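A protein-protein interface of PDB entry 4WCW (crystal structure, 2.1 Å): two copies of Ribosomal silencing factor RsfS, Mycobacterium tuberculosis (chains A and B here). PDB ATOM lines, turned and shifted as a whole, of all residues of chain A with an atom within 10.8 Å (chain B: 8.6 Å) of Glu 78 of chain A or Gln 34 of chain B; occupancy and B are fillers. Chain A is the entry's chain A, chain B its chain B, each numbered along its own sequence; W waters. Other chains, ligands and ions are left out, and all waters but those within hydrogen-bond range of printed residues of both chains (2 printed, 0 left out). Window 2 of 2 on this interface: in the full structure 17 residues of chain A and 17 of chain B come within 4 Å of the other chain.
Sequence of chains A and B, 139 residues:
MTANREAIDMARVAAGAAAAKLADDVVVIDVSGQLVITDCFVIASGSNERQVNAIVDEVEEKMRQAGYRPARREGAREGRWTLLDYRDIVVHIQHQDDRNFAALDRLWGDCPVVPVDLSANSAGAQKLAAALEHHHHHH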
ATOM      1  N   GLU A  49      -8.255  -2.903 -34.818  1.00  0.00           N
ATOM      2  CA  GLU A  49      -9.066  -2.629 -33.632  1.00  0.00           C
ATOM      3  C   GLU A  49     -10.227  -1.679 -33.926  1.00  0.00           C
ATOM      4  O   GLU A  49     -11.275  -1.739 -33.276  1.00  0.00           O
ATOM      5  CB  GLU A  49      -8.182  -2.077 -32.508  1.00  0.00           C
ATOM      6  CG  GLU A  49      -8.848  -2.035 -31.136  1.00  0.00           C
ATOM      7  CD  GLU A  49      -7.839  -2.004 -30.007  1.00  0.00           C
ATOM      8  OE1 GLU A  49      -6.629  -1.930 -30.300  1.00  0.00           O
ATOM      9  OE2 GLU A  49      -8.252  -2.060 -28.831  1.00  0.00           O
ATOM     10  N   ARG A  72     -25.329  -8.064 -22.230  1.00  0.00           N
ATOM     11  CA  ARG A  72     -24.410  -7.983 -21.106  1.00  0.00           C
ATOM     12  C   ARG A  72     -23.043  -8.079 -21.757  1.00  0.00           C
ATOM     13  O   ARG A  72     -22.783  -9.009 -22.517  1.00  0.00           O
ATOM     14  CB  ARG A  72     -24.650  -9.135 -20.124  1.00  0.00           C
ATOM     15  CG  ARG A  72     -23.873  -9.062 -18.793  1.00  0.00           C
ATOM     16  CD  ARG A  72     -22.391  -9.431 -18.937  1.00  0.00           C
ATOM     17  NE  ARG A  72     -21.861 -10.127 -17.764  1.00  0.00           N
ATOM     18  CZ  ARG A  72     -20.616 -10.004 -17.308  1.00  0.00           C
ATOM     19  NH1 ARG A  72     -19.757  -9.196 -17.910  1.00  0.00           N
ATOM     20  NH2 ARG A  72     -20.230 -10.687 -16.240  1.00  0.00           N
ATOM     21  N   GLU A  74     -18.660  -7.883 -22.041  1.00  0.00           N
ATOM     22  CA  GLU A  74     -17.374  -8.125 -21.395  1.00  0.00           C
ATOM     23  C   GLU A  74     -16.233  -7.992 -22.398  1.00  0.00           C
ATOM     24  O   GLU A  74     -16.416  -8.197 -23.608  1.00  0.00           O
ATOM     25  CB  GLU A  74     -17.349  -9.497 -20.718  1.00  0.00           C
ATOM     26  CG  GLU A  74     -16.177  -9.710 -19.760  1.00  0.00           C
ATOM     27  CD  GLU A  74     -16.132  -8.684 -18.643  1.00  0.00           C
ATOM     28  OE1 GLU A  74     -16.701  -8.955 -17.562  1.00  0.00           O
ATOM     29  OE2 GLU A  74     -15.518  -7.606 -18.839  1.00  0.00           O
ATOM     30  N   GLY A  75     -15.066  -7.614 -21.890  1.00  0.00           N
ATOM     31  CA  GLY A  75     -13.865  -7.500 -22.691  1.00  0.00           C
ATOM     32  C   GLY A  75     -12.674  -7.410 -21.758  1.00  0.00           C
ATOM     33  O   GLY A  75     -12.838  -7.228 -20.551  1.00  0.00           O
ATOM     34  N   ALA A  76     -11.474  -7.565 -22.304  1.00  0.00           N
ATOM     35  CA  ALA A  76     -10.261  -7.394 -21.514  1.00  0.00           C
ATOM     36  C   ALA A  76      -9.828  -5.946 -21.624  1.00  0.00           C
ATOM     37  O   ALA A  76      -9.905  -5.356 -22.702  1.00  0.00           O
ATOM     38  CB  ALA A  76      -9.166  -8.318 -22.007  1.00  0.00           C
ATOM     39  N   ARG A  77      -9.380  -5.372 -20.514  1.00  0.00           N
ATOM     40  CA  ARG A  77      -8.947  -3.983 -20.518  1.00  0.00           C
ATOM     41  C   ARG A  77      -7.725  -3.807 -21.417  1.00  0.00           C
ATOM     42  O   ARG A  77      -7.576  -2.773 -22.068  1.00  0.00           O
ATOM     43  CB  ARG A  77      -8.647  -3.515 -19.095  1.00  0.00           C
ATOM     44  CG  ARG A  77      -9.828  -3.644 -18.149  1.00  0.00           C
ATOM     45  CD  ARG A  77      -9.447  -3.310 -16.713  1.00  0.00           C
ATOM     46  NE  ARG A  77      -9.235  -1.875 -16.509  1.00  0.00           N
ATOM     47  CZ  ARG A  77      -9.142  -1.302 -15.316  1.00  0.00           C
ATOM     48  NH1 ARG A  77      -9.247  -2.048 -14.222  1.00  0.00           N
ATOM     49  NH2 ARG A  77      -8.945   0.009 -15.213  1.00  0.00           N
ATOM     50  N   GLU A  78      -6.868  -4.826 -21.464  1.00  0.00           N
ATOM     51  CA  GLU A  78      -5.669  -4.789 -22.301  1.00  0.00           C
ATOM     52  C   GLU A  78      -5.833  -5.619 -23.570  1.00  0.00           C
ATOM     53  O   GLU A  78      -4.905  -5.720 -24.375  1.00  0.00           O
ATOM     54  CB  GLU A  78      -4.457  -5.319 -21.535  1.00  0.00           C
ATOM     55  CG  GLU A  78      -4.208  -4.687 -20.184  1.00  0.00           C
ATOM     56  CD  GLU A  78      -3.115  -5.410 -19.421  1.00  0.00           C
ATOM     57  OE1 GLU A  78      -2.055  -5.689 -20.026  1.00  0.00           O
ATOM     58  OE2 GLU A  78      -3.323  -5.711 -18.227  1.00  0.00           O
ATOM     59  N   GLY A  79      -7.000  -6.228 -23.748  1.00  0.00           N
ATOM     60  CA  GLY A  79      -7.213  -7.097 -24.892  1.00  0.00           C
ATOM     61  C   GLY A  79      -7.924  -6.407 -26.035  1.00  0.00           C
ATOM     62  O   GLY A  79      -8.307  -5.244 -25.926  1.00  0.00           O
ATOM     63  N   ARG A  80      -8.111  -7.131 -27.133  1.00  0.00           N
ATOM     64  CA  ARG A  80      -8.826  -6.594 -28.287  1.00  0.00           C
ATOM     65  C   ARG A  80     -10.011  -7.492 -28.659  1.00  0.00           C
ATOM     66  O   ARG A  80     -10.257  -7.779 -29.838  1.00  0.00           O
ATOM     67  CB  ARG A  80      -7.866  -6.405 -29.466  1.00  0.00           C
ATOM     68  CG  ARG A  80      -6.671  -5.509 -29.142  1.00  0.00           C
ATOM     69  CD  ARG A  80      -5.763  -5.313 -30.340  1.00  0.00           C
ATOM     70  NE  ARG A  80      -5.061  -6.537 -30.723  1.00  0.00           N
ATOM     71  CZ  ARG A  80      -4.117  -6.584 -31.657  1.00  0.00           C
ATOM     72  NH1 ARG A  80      -3.767  -5.474 -32.287  1.00  0.00           N
ATOM     73  NH2 ARG A  80      -3.519  -7.729 -31.959  1.00  0.00           N
ATOM     74  N   TRP A  81     -10.733  -7.937 -27.632  1.00  0.00           N
ATOM     75  CA  TRP A  81     -11.958  -8.703 -27.825  1.00  0.00           C
ATOM     76  C   TRP A  81     -13.128  -8.068 -27.092  1.00  0.00           C
ATOM     77  O   TRP A  81     -12.935  -7.275 -26.167  1.00  0.00           O
ATOM     78  CB  TRP A  81     -11.780 -10.161 -27.388  1.00  0.00           C
ATOM     79  CG  TRP A  81     -11.390 -10.368 -25.948  1.00  0.00           C
ATOM     80  CD1 TRP A  81     -10.127 -10.392 -25.436  1.00  0.00           C
ATOM     81  CD2 TRP A  81     -12.273 -10.635 -24.846  1.00  0.00           C
ATOM     82  NE1 TRP A  81     -10.172 -10.640 -24.084  1.00  0.00           N
ATOM     83  CE2 TRP A  81     -11.479 -10.791 -23.700  1.00  0.00           C
ATOM     84  CE3 TRP A  81     -13.659 -10.748 -24.724  1.00  0.00           C
ATOM     85  CZ2 TRP A  81     -12.024 -11.056 -22.440  1.00  0.00           C
ATOM     86  CZ3 TRP A  81     -14.201 -11.010 -23.475  1.00  0.00           C
ATOM     87  CH2 TRP A  81     -13.385 -11.159 -22.349  1.00  0.00           C
ATOM     88  N   THR A  82     -14.339  -8.398 -27.532  1.00  0.00           N
ATOM     89  CA  THR A  82     -15.553  -8.005 -26.823  1.00  0.00           C
ATOM     90  C   THR A  82     -16.552  -9.144 -26.873  1.00  0.00           C
ATOM     91  O   THR A  82     -16.723  -9.796 -27.909  1.00  0.00           O
ATOM     92  CB  THR A  82     -16.185  -6.729 -27.406  1.00  0.00           C
ATOM     93  OG1 THR A  82     -15.284  -5.630 -27.238  1.00  0.00           O
ATOM     94  CG2 THR A  82     -17.506  -6.398 -26.701  1.00  0.00           C
ATOM     95  N   GLN A  94     -13.319 -10.481 -32.041  1.00  0.00           N
ATOM     96  CA  GLN A  94     -11.910 -10.340 -31.665  1.00  0.00           C
ATOM     97  C   GLN A  94     -11.014  -9.953 -32.830  1.00  0.00           C
ATOM     98  O   GLN A  94     -11.294 -10.283 -33.983  1.00  0.00           O
ATOM     99  CB  GLN A  94     -11.391 -11.627 -31.016  1.00  0.00           C
ATOM    100  CG  GLN A  94     -10.016 -11.484 -30.349  1.00  0.00           C
ATOM    101  CD  GLN A  94      -9.678 -12.659 -29.453  1.00  0.00           C
ATOM    102  OE1 GLN A  94     -10.197 -13.756 -29.634  1.00  0.00           O
ATOM    103  NE2 GLN A  94      -8.813 -12.431 -28.472  1.00  0.00           N
ATOM    104  N   HIS A  95      -9.936  -9.238 -32.525  1.00  0.00           N
ATOM    105  CA  HIS A  95      -8.905  -8.982 -33.518  1.00  0.00           C
ATOM    106  C   HIS A  95      -8.360 -10.335 -33.936  1.00  0.00           C
ATOM    107  O   HIS A  95      -8.060 -11.165 -33.082  1.00  0.00           O
ATOM    108  CB  HIS A  95      -7.792  -8.128 -32.920  1.00  0.00           C
ATOM    109  CG  HIS A  95      -6.856  -7.556 -33.932  1.00  0.00           C
ATOM    110  ND1 HIS A  95      -6.135  -8.341 -34.815  1.00  0.00           N
ATOM    111  CD2 HIS A  95      -6.497  -6.279 -34.200  1.00  0.00           C
ATOM    112  CE1 HIS A  95      -5.391  -7.571 -35.581  1.00  0.00           C
ATOM    113  NE2 HIS A  95      -5.593  -6.309 -35.230  1.00  0.00           N
ATOM    114  N   ASP A  98      -5.234 -11.900 -32.431  1.00  0.00           N
ATOM    115  CA  ASP A  98      -5.281 -12.349 -31.038  1.00  0.00           C
ATOM    116  C   ASP A  98      -6.002 -13.685 -30.870  1.00  0.00           C
ATOM    117  O   ASP A  98      -5.905 -14.325 -29.824  1.00  0.00           O
ATOM    118  CB  ASP A  98      -5.962 -11.296 -30.154  1.00  0.00           C
ATOM    119  CG  ASP A  98      -5.253  -9.960 -30.182  1.00  0.00           C
ATOM    120  OD1 ASP A  98      -4.122  -9.896 -30.701  1.00  0.00           O
ATOM    121  OD2 ASP A  98      -5.825  -8.973 -29.678  1.00  0.00           O
ATOM    122  N   ILE B  29     -11.261 -14.988  -6.843  1.00  0.00           N
ATOM    123  CA  ILE B  29     -10.240 -14.358  -7.680  1.00  0.00           C
ATOM    124  C   ILE B  29     -10.641 -12.947  -8.093  1.00  0.00           C
ATOM    125  O   ILE B  29     -11.682 -12.752  -8.723  1.00  0.00           O
ATOM    126  CB  ILE B  29      -9.970 -15.183  -8.950  1.00  0.00           C
ATOM    127  CG1 ILE B  29      -9.601 -16.619  -8.576  1.00  0.00           C
ATOM    128  CG2 ILE B  29      -8.862 -14.549  -9.780  1.00  0.00           C
ATOM    129  CD1 ILE B  29      -9.523 -17.575  -9.747  1.00  0.00           C
ATOM    130  N   ASP B  30      -9.809 -11.974  -7.738  1.00  0.00           N
ATOM    131  CA  ASP B  30     -10.019 -10.583  -8.132  1.00  0.00           C
ATOM    132  C   ASP B  30      -9.531 -10.386  -9.565  1.00  0.00           C
ATOM    133  O   ASP B  30      -8.329 -10.385  -9.817  1.00  0.00           O
ATOM    134  CB  ASP B  30      -9.248  -9.658  -7.180  1.00  0.00           C
ATOM    135  CG  ASP B  30      -9.444  -8.173  -7.485  1.00  0.00           C
ATOM    136  OD1 ASP B  30      -9.985  -7.807  -8.556  1.00  0.00           O
ATOM    137  OD2 ASP B  30      -9.034  -7.356  -6.633  1.00  0.00           O
ATOM    138  N   VAL B  31     -10.460 -10.209 -10.499  1.00  0.00           N
ATOM    139  CA  VAL B  31     -10.089  -9.994 -11.897  1.00  0.00           C
ATOM    140  C   VAL B  31     -10.370  -8.563 -12.351  1.00  0.00           C
ATOM    141  O   VAL B  31     -10.346  -8.265 -13.550  1.00  0.00           O
ATOM    142  CB  VAL B  31     -10.816 -10.977 -12.831  1.00  0.00           C
ATOM    143  CG1 VAL B  31     -10.372 -12.408 -12.548  1.00  0.00           C
ATOM    144  CG2 VAL B  31     -12.332 -10.822 -12.693  1.00  0.00           C
ATOM    145  N   SER B  32     -10.632  -7.686 -11.383  1.00  0.00           N
ATOM    146  CA  SER B  32     -10.964  -6.285 -11.652  1.00  0.00           C
ATOM    147  C   SER B  32      -9.872  -5.559 -12.430  1.00  0.00           C
ATOM    148  O   SER B  32     -10.149  -4.628 -13.192  1.00  0.00           O
ATOM    149  CB  SER B  32     -11.228  -5.538 -10.344  1.00  0.00           C
ATOM    150  OG  SER B  32     -10.047  -5.420  -9.566  1.00  0.00           O
ATOM    151  N   GLY B  33      -8.628  -5.985 -12.236  1.00  0.00           N
ATOM    152  CA  GLY B  33      -7.509  -5.370 -12.925  1.00  0.00           C
ATOM    153  C   GLY B  33      -7.483  -5.744 -14.393  1.00  0.00           C
ATOM    154  O   GLY B  33      -6.939  -5.008 -15.218  1.00  0.00           O
ATOM    155  N   GLN B  34      -8.092  -6.886 -14.714  1.00  0.00           N
ATOM    156  CA  GLN B  34      -8.030  -7.463 -16.058  1.00  0.00           C
ATOM    157  C   GLN B  34      -9.254  -7.163 -16.924  1.00  0.00           C
ATOM    158  O   GLN B  34      -9.123  -6.810 -18.101  1.00  0.00           O
ATOM    159  CB  GLN B  34      -7.864  -8.984 -15.962  1.00  0.00           C
ATOM    160  CG  GLN B  34      -6.507  -9.459 -15.459  1.00  0.00           C
ATOM    161  CD  GLN B  34      -5.470  -9.488 -16.555  1.00  0.00           C
ATOM    162  OE1 GLN B  34      -4.888  -8.464 -16.901  1.00  0.00           O
ATOM    163  NE2 GLN B  34      -5.247 -10.663 -17.126  1.00  0.00           N
ATOM    164  N   LEU B  35     -10.440  -7.328 -16.342  1.00  0.00           N
ATOM    165  CA  LEU B  35     -11.687  -7.240 -17.098  1.00  0.00           C
ATOM    166  C   LEU B  35     -12.372  -5.885 -16.957  1.00  0.00           C
ATOM    167  O   LEU B  35     -12.098  -5.132 -16.024  1.00  0.00           O
ATOM    168  CB  LEU B  35     -12.648  -8.357 -16.686  1.00  0.00           C
ATOM    169  CG  LEU B  35     -12.244  -9.798 -16.998  1.00  0.00           C
ATOM    170  CD1 LEU B  35     -13.419 -10.744 -16.755  1.00  0.00           C
ATOM    171  CD2 LEU B  35     -11.732  -9.929 -18.422  1.00  0.00           C
ATOM    172  N   VAL B  36     -13.260  -5.580 -17.900  1.00  0.00           N
ATOM    173  CA  VAL B  36     -13.997  -4.314 -17.915  1.00  0.00           C
ATOM    174  C   VAL B  36     -15.185  -4.316 -16.953  1.00  0.00           C
ATOM    175  O   VAL B  36     -15.417  -3.341 -16.237  1.00  0.00           O
ATOM    176  CB  VAL B  36     -14.501  -3.988 -19.344  1.00  0.00           C
ATOM    177  CG1 VAL B  36     -15.346  -2.730 -19.344  1.00  0.00           C
ATOM    178  CG2 VAL B  36     -13.329  -3.832 -20.302  1.00  0.00           C
ATOM    179  N   ILE B  37     -15.926  -5.420 -16.932  1.00  0.00           N
ATOM    180  CA  ILE B  37     -17.176  -5.493 -16.179  1.00  0.00           C
ATOM    181  C   ILE B  37     -17.088  -6.322 -14.891  1.00  0.00           C
ATOM    182  O   ILE B  37     -17.326  -5.816 -13.793  1.00  0.00           O
ATOM    183  CB  ILE B  37     -18.307  -6.042 -17.062  1.00  0.00           C
ATOM    184  CG1 ILE B  37     -18.503  -5.143 -18.285  1.00  0.00           C
ATOM    185  CG2 ILE B  37     -19.596  -6.177 -16.256  1.00  0.00           C
ATOM    186  CD1 ILE B  37     -18.926  -3.719 -17.941  1.00  0.00           C
ATOM    187  N   THR B  38     -16.768  -7.602 -15.039  1.00  0.00           N
ATOM    188  CA  THR B  38     -16.629  -8.512 -13.902  1.00  0.00           C
ATOM    189  C   THR B  38     -15.482  -8.103 -12.983  1.00  0.00           C
ATOM    190  O   THR B  38     -14.382  -7.812 -13.451  1.00  0.00           O
ATOM    191  CB  THR B  38     -16.381  -9.952 -14.389  1.00  0.00           C
ATOM    192  OG1 THR B  38     -17.530 -10.411 -15.116  1.00  0.00           O
ATOM    193  CG2 THR B  38     -16.118 -10.889 -13.216  1.00  0.00           C
ATOM    194  N   ASP B  39     -15.730  -8.091 -11.676  1.00  0.00           N
ATOM    195  CA  ASP B  39     -14.672  -7.770 -10.719  1.00  0.00           C
ATOM    196  C   ASP B  39     -14.090  -8.990 -10.007  1.00  0.00           C
ATOM    197  O   ASP B  39     -12.890  -9.037  -9.734  1.00  0.00           O
ATOM    198  CB  ASP B  39     -15.146  -6.727  -9.707  1.00  0.00           C
ATOM    199  CG  ASP B  39     -14.871  -5.314 -10.170  1.00  0.00           C
ATOM    200  OD1 ASP B  39     -14.158  -5.160 -11.187  1.00  0.00           O
ATOM    201  OD2 ASP B  39     -15.358  -4.363  -9.524  1.00  0.00           O
ATOM    202  N   PHE B  41     -14.173 -13.508  -9.632  1.00  0.00           N
ATOM    203  CA  PHE B  41     -14.637 -14.850  -9.943  1.00  0.00           C
ATOM    204  C   PHE B  41     -14.686 -15.618  -8.643  1.00  0.00           C
ATOM    205  O   PHE B  41     -13.855 -15.400  -7.758  1.00  0.00           O
ATOM    206  CB  PHE B  41     -13.671 -15.560 -10.889  1.00  0.00           C
ATOM    207  CG  PHE B  41     -13.768 -15.103 -12.308  1.00  0.00           C
ATOM    208  CD1 PHE B  41     -14.982 -14.706 -12.844  1.00  0.00           C
ATOM    209  CD2 PHE B  41     -12.648 -15.069 -13.108  1.00  0.00           C
ATOM    210  CE1 PHE B  41     -15.072 -14.286 -14.159  1.00  0.00           C
ATOM    211  CE2 PHE B  41     -12.739 -14.652 -14.411  1.00  0.00           C
ATOM    212  CZ  PHE B  41     -13.945 -14.261 -14.941  1.00  0.00           C
ATOM    213  N   ARG B 106      -2.182 -19.940 -15.912  1.00  0.00           N
ATOM    214  CA  ARG B 106      -1.643 -19.176 -17.040  1.00  0.00           C
ATOM    215  C   ARG B 106      -2.534 -17.996 -17.416  1.00  0.00           C
ATOM    216  O   ARG B 106      -2.220 -17.242 -18.337  1.00  0.00           O
ATOM    217  CB  ARG B 106      -1.460 -20.070 -18.274  1.00  0.00           C
ATOM    218  CG  ARG B 106      -2.757 -20.411 -19.009  1.00  0.00           C
ATOM    219  CD  ARG B 106      -2.496 -21.261 -20.250  1.00  0.00           C
ATOM    220  NE  ARG B 106      -3.692 -21.968 -20.707  1.00  0.00           N
ATOM    221  CZ  ARG B 106      -3.825 -23.291 -20.705  1.00  0.00           C
ATOM    222  NH1 ARG B 106      -2.834 -24.060 -20.278  1.00  0.00           N
ATOM    223  NH2 ARG B 106      -4.944 -23.851 -21.140  1.00  0.00           N
ATOM    224  N   LEU B 107      -3.640 -17.833 -16.703  1.00  0.00           N
ATOM    225  CA  LEU B 107      -4.673 -16.916 -17.146  1.00  0.00           C
ATOM    226  C   LEU B 107      -5.164 -15.961 -16.040  1.00  0.00           C
ATOM    227  O   LEU B 107      -5.265 -14.756 -16.276  1.00  0.00           O
ATOM    228  CB  LEU B 107      -5.785 -17.731 -17.828  1.00  0.00           C
ATOM    229  CG  LEU B 107      -7.167 -17.229 -18.252  1.00  0.00           C
ATOM    230  CD1 LEU B 107      -7.589 -17.931 -19.501  1.00  0.00           C
ATOM    231  CD2 LEU B 107      -8.194 -17.499 -17.150  1.00  0.00           C
ATOM    232  N   TRP B 108      -5.435 -16.473 -14.837  1.00  0.00           N
ATOM    233  CA  TRP B 108      -5.615 -15.586 -13.670  1.00  0.00           C
ATOM    234  C   TRP B 108      -4.511 -15.740 -12.616  1.00  0.00           C
ATOM    235  O   TRP B 108      -4.769 -15.594 -11.419  1.00  0.00           O
ATOM    236  CB  TRP B 108      -6.969 -15.778 -12.972  1.00  0.00           C
ATOM    237  CG  TRP B 108      -8.168 -15.768 -13.862  1.00  0.00           C
ATOM    238  CD1 TRP B 108      -9.131 -16.731 -13.935  1.00  0.00           C
ATOM    239  CD2 TRP B 108      -8.545 -14.751 -14.801  1.00  0.00           C
ATOM    240  NE1 TRP B 108     -10.079 -16.378 -14.858  1.00  0.00           N
ATOM    241  CE2 TRP B 108      -9.741 -15.168 -15.408  1.00  0.00           C
ATOM    242  CE3 TRP B 108      -7.987 -13.530 -15.187  1.00  0.00           C
ATOM    243  CZ2 TRP B 108     -10.383 -14.415 -16.394  1.00  0.00           C
ATOM    244  CZ3 TRP B 108      -8.632 -12.780 -16.153  1.00  0.00           C
ATOM    245  CH2 TRP B 108      -9.820 -13.219 -16.739  1.00  0.00           C
ATOM    246  N   GLY B 109      -3.286 -16.021 -13.050  1.00  0.00           N
ATOM    247  CA  GLY B 109      -2.191 -16.261 -12.122  1.00  0.00           C
ATOM    248  C   GLY B 109      -1.615 -15.011 -11.489  1.00  0.00           C
ATOM    249  O   GLY B 109      -1.122 -15.051 -10.362  1.00  0.00           O
ATOM    250  N   ASP B 110      -1.681 -13.902 -12.216  1.00  0.00           N
ATOM    251  CA  ASP B 110      -1.122 -12.642 -11.743  1.00  0.00           C
ATOM    252  C   ASP B 110      -2.152 -11.866 -10.926  1.00  0.00           C
ATOM    253  O   ASP B 110      -1.814 -10.915 -10.216  1.00  0.00           O
ATOM    254  CB  ASP B 110      -0.639 -11.808 -12.929  1.00  0.00           C
ATOM    255  CG  ASP B 110       0.024 -12.654 -14.000  1.00  0.00           C
ATOM    256  OD1 ASP B 110       0.689 -13.654 -13.651  1.00  0.00           O
ATOM    257  OD2 ASP B 110      -0.127 -12.324 -15.197  1.00  0.00           O
ATOM    258  N   CYS B 111      -3.410 -12.282 -11.037  1.00  0.00           N
ATOM    259  CA  CYS B 111      -4.495 -11.705 -10.252  1.00  0.00           C
ATOM    260  C   CYS B 111      -4.410 -12.196  -8.812  1.00  0.00           C
ATOM    261  O   CYS B 111      -4.028 -13.343  -8.568  1.00  0.00           O
ATOM    262  CB  CYS B 111      -5.846 -12.113 -10.839  1.00  0.00           C
ATOM    263  SG  CYS B 111      -6.036 -11.808 -12.603  1.00  0.00           S
ATOM    264  N   PRO B 112      -4.765 -11.329  -7.850  1.00  0.00           N
ATOM    265  CA  PRO B 112      -4.764 -11.727  -6.438  1.00  0.00           C
ATOM    266  C   PRO B 112      -5.851 -12.764  -6.201  1.00  0.00           C
ATOM    267  O   PRO B 112      -6.915 -12.663  -6.809  1.00  0.00           O
ATOM    268  CB  PRO B 112      -5.119 -10.430  -5.703  1.00  0.00           C
ATOM    269  CG  PRO B 112      -4.909  -9.330  -6.692  1.00  0.00           C
ATOM    270  CD  PRO B 112      -5.194  -9.931  -8.027  1.00  0.00           C
HETATM  271  O   HOH W   1      -6.814  -6.954 -19.785  1.00  0.00           O
HETATM  272  O   HOH W   2      -4.940  -3.888 -16.930  1.00  0.00           O
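No position is printed for both chains. Of the 15 pairs that touch across the chains among the printed residues, none has its exchanged pair printed and touching as well.
Of the 19 printed residues of chain B, 7 touch a printed residue of chain A. Hydrophobic or aromatic side chains of chain B that line the printed part of chain A: Leu 35, Val 36 and Ile 37.
Among the printed residues, pairs that only touch across the chains: Arg 77 of chain A with Leu 35 of chain B, Arg 77 of chain A with Gly 33 of chain B, Arg 72 of chain A with Ile 37 of chain B, Gly 75 of chain A with Leu 35 of chain B, Ala 76 of chain A with Gln 34 of chain B, Glu 74 of chain A with Leu 35 of chain B and Arg 77 of chain A with Val 36 of chain B.
The guanidinium group (NH2) of Arg 72 of chain A lies within hydrogen-bond range of the side-chain hydroxyl (OG1) of Thr 38 of chain B (2.9 Å). The side-chain carboxylate (OE2) of Glu 74 of chain A sits at hydrogen-bond distance from the backbone NH (N) of Val 36 of chain B, 3.2 Å away. OE2 of Glu 74 of chain A lies within hydrogen-bond range of N of Ile 37 of chain B (2.9 Å). The side-chain carboxylate (OE1) of Glu 74 of chain A sits at hydrogen-bond distance from the backbone NH (N) of Thr 38 of chain B. O of Gly 75 of chain A is in hydrogen-bond range of N of Val 36 of chain B (3.1 Å). The backbone carbonyl oxygen (O) of Ser 32 of chain B is in hydrogen-bond range of the guanidinium group (NH1) of Arg 77 of chain A. O of Gln 34 of chain B is in hydrogen-bond range of N of Arg 77 of chain A (2.8 Å). The side-chain carboxylate of Glu 78 of chain A sits close to the side-chain amide oxygen of Gln 34 of chain B, at 3.4 Å.
Water W1 lies within hydrogen-bond range of N of Glu 78 of chain A (2.7 Å), O of Gln 34 of chain B (2.9 Å) and N of Arg 77 of chain A (3.1 Å). Water W2 bridges the side-chain carboxylate of Glu 78 of chain A (2.8 Å) and the backbone carbonyl oxygen of Gly 33 of chain B (2.9 Å).
NH1 of Arg 72 of chain A lies within salt-bridge range of OE1 of Glu 74 of chain A (3.1 Å). OD1 of Asp 30 of chain B is in hydrogen-bond range of OG of Ser 32 of chain B (2.6 Å). The backbone carbonyl oxygen of Asp 39 of chain B is in hydrogen-bond range of the backbone NH of Ser 32 of chain B, 3.1 Å away.
Of chain B, only Gln 34 comes within 4 Å of Glu 78 of chain A. Of the printed residues of chain A, Gln 34 of chain B touches Ala 76 (3.6 Å), Arg 77 (2.8 Å) and Glu 78 (3.4 Å). No residue of chain B comes within 4 Å of Gly 79 of chain A. No residue of chain A comes within 4 Å of Val 31 of chain B. Of chain A, only Arg 77 (2.9 Å) comes within 4 Å of Ser 32 of chain B. Of the printed residues of chain B, Glu 74 of chain A touches Leu 35 (3.7 Å), Val 36 (3.2 Å), Ile 37 (2.9 Å) and Thr 38 (2.9 Å). Of the printed residues of chain A, Ile 37 of chain B touches Arg 72 (3.4 Å) and Glu 74 (2.9 Å). Of the printed residues of chain B, Gly 75 of chain A touches Leu 35 and Val 36. Of the printed residues of chain B, Arg 77 of chain A touches Ser 32, Gly 33, Gln 34, Leu 35 and Val 36. Asp 39 of chain B touches none of the printed residues of chain A. Asp 110 of chain B touches none of the printed residues of chain A. The nearest residue of chain B that does not touch Glu 78 of chain A is Gly 33 of chain B (4.8 Å).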
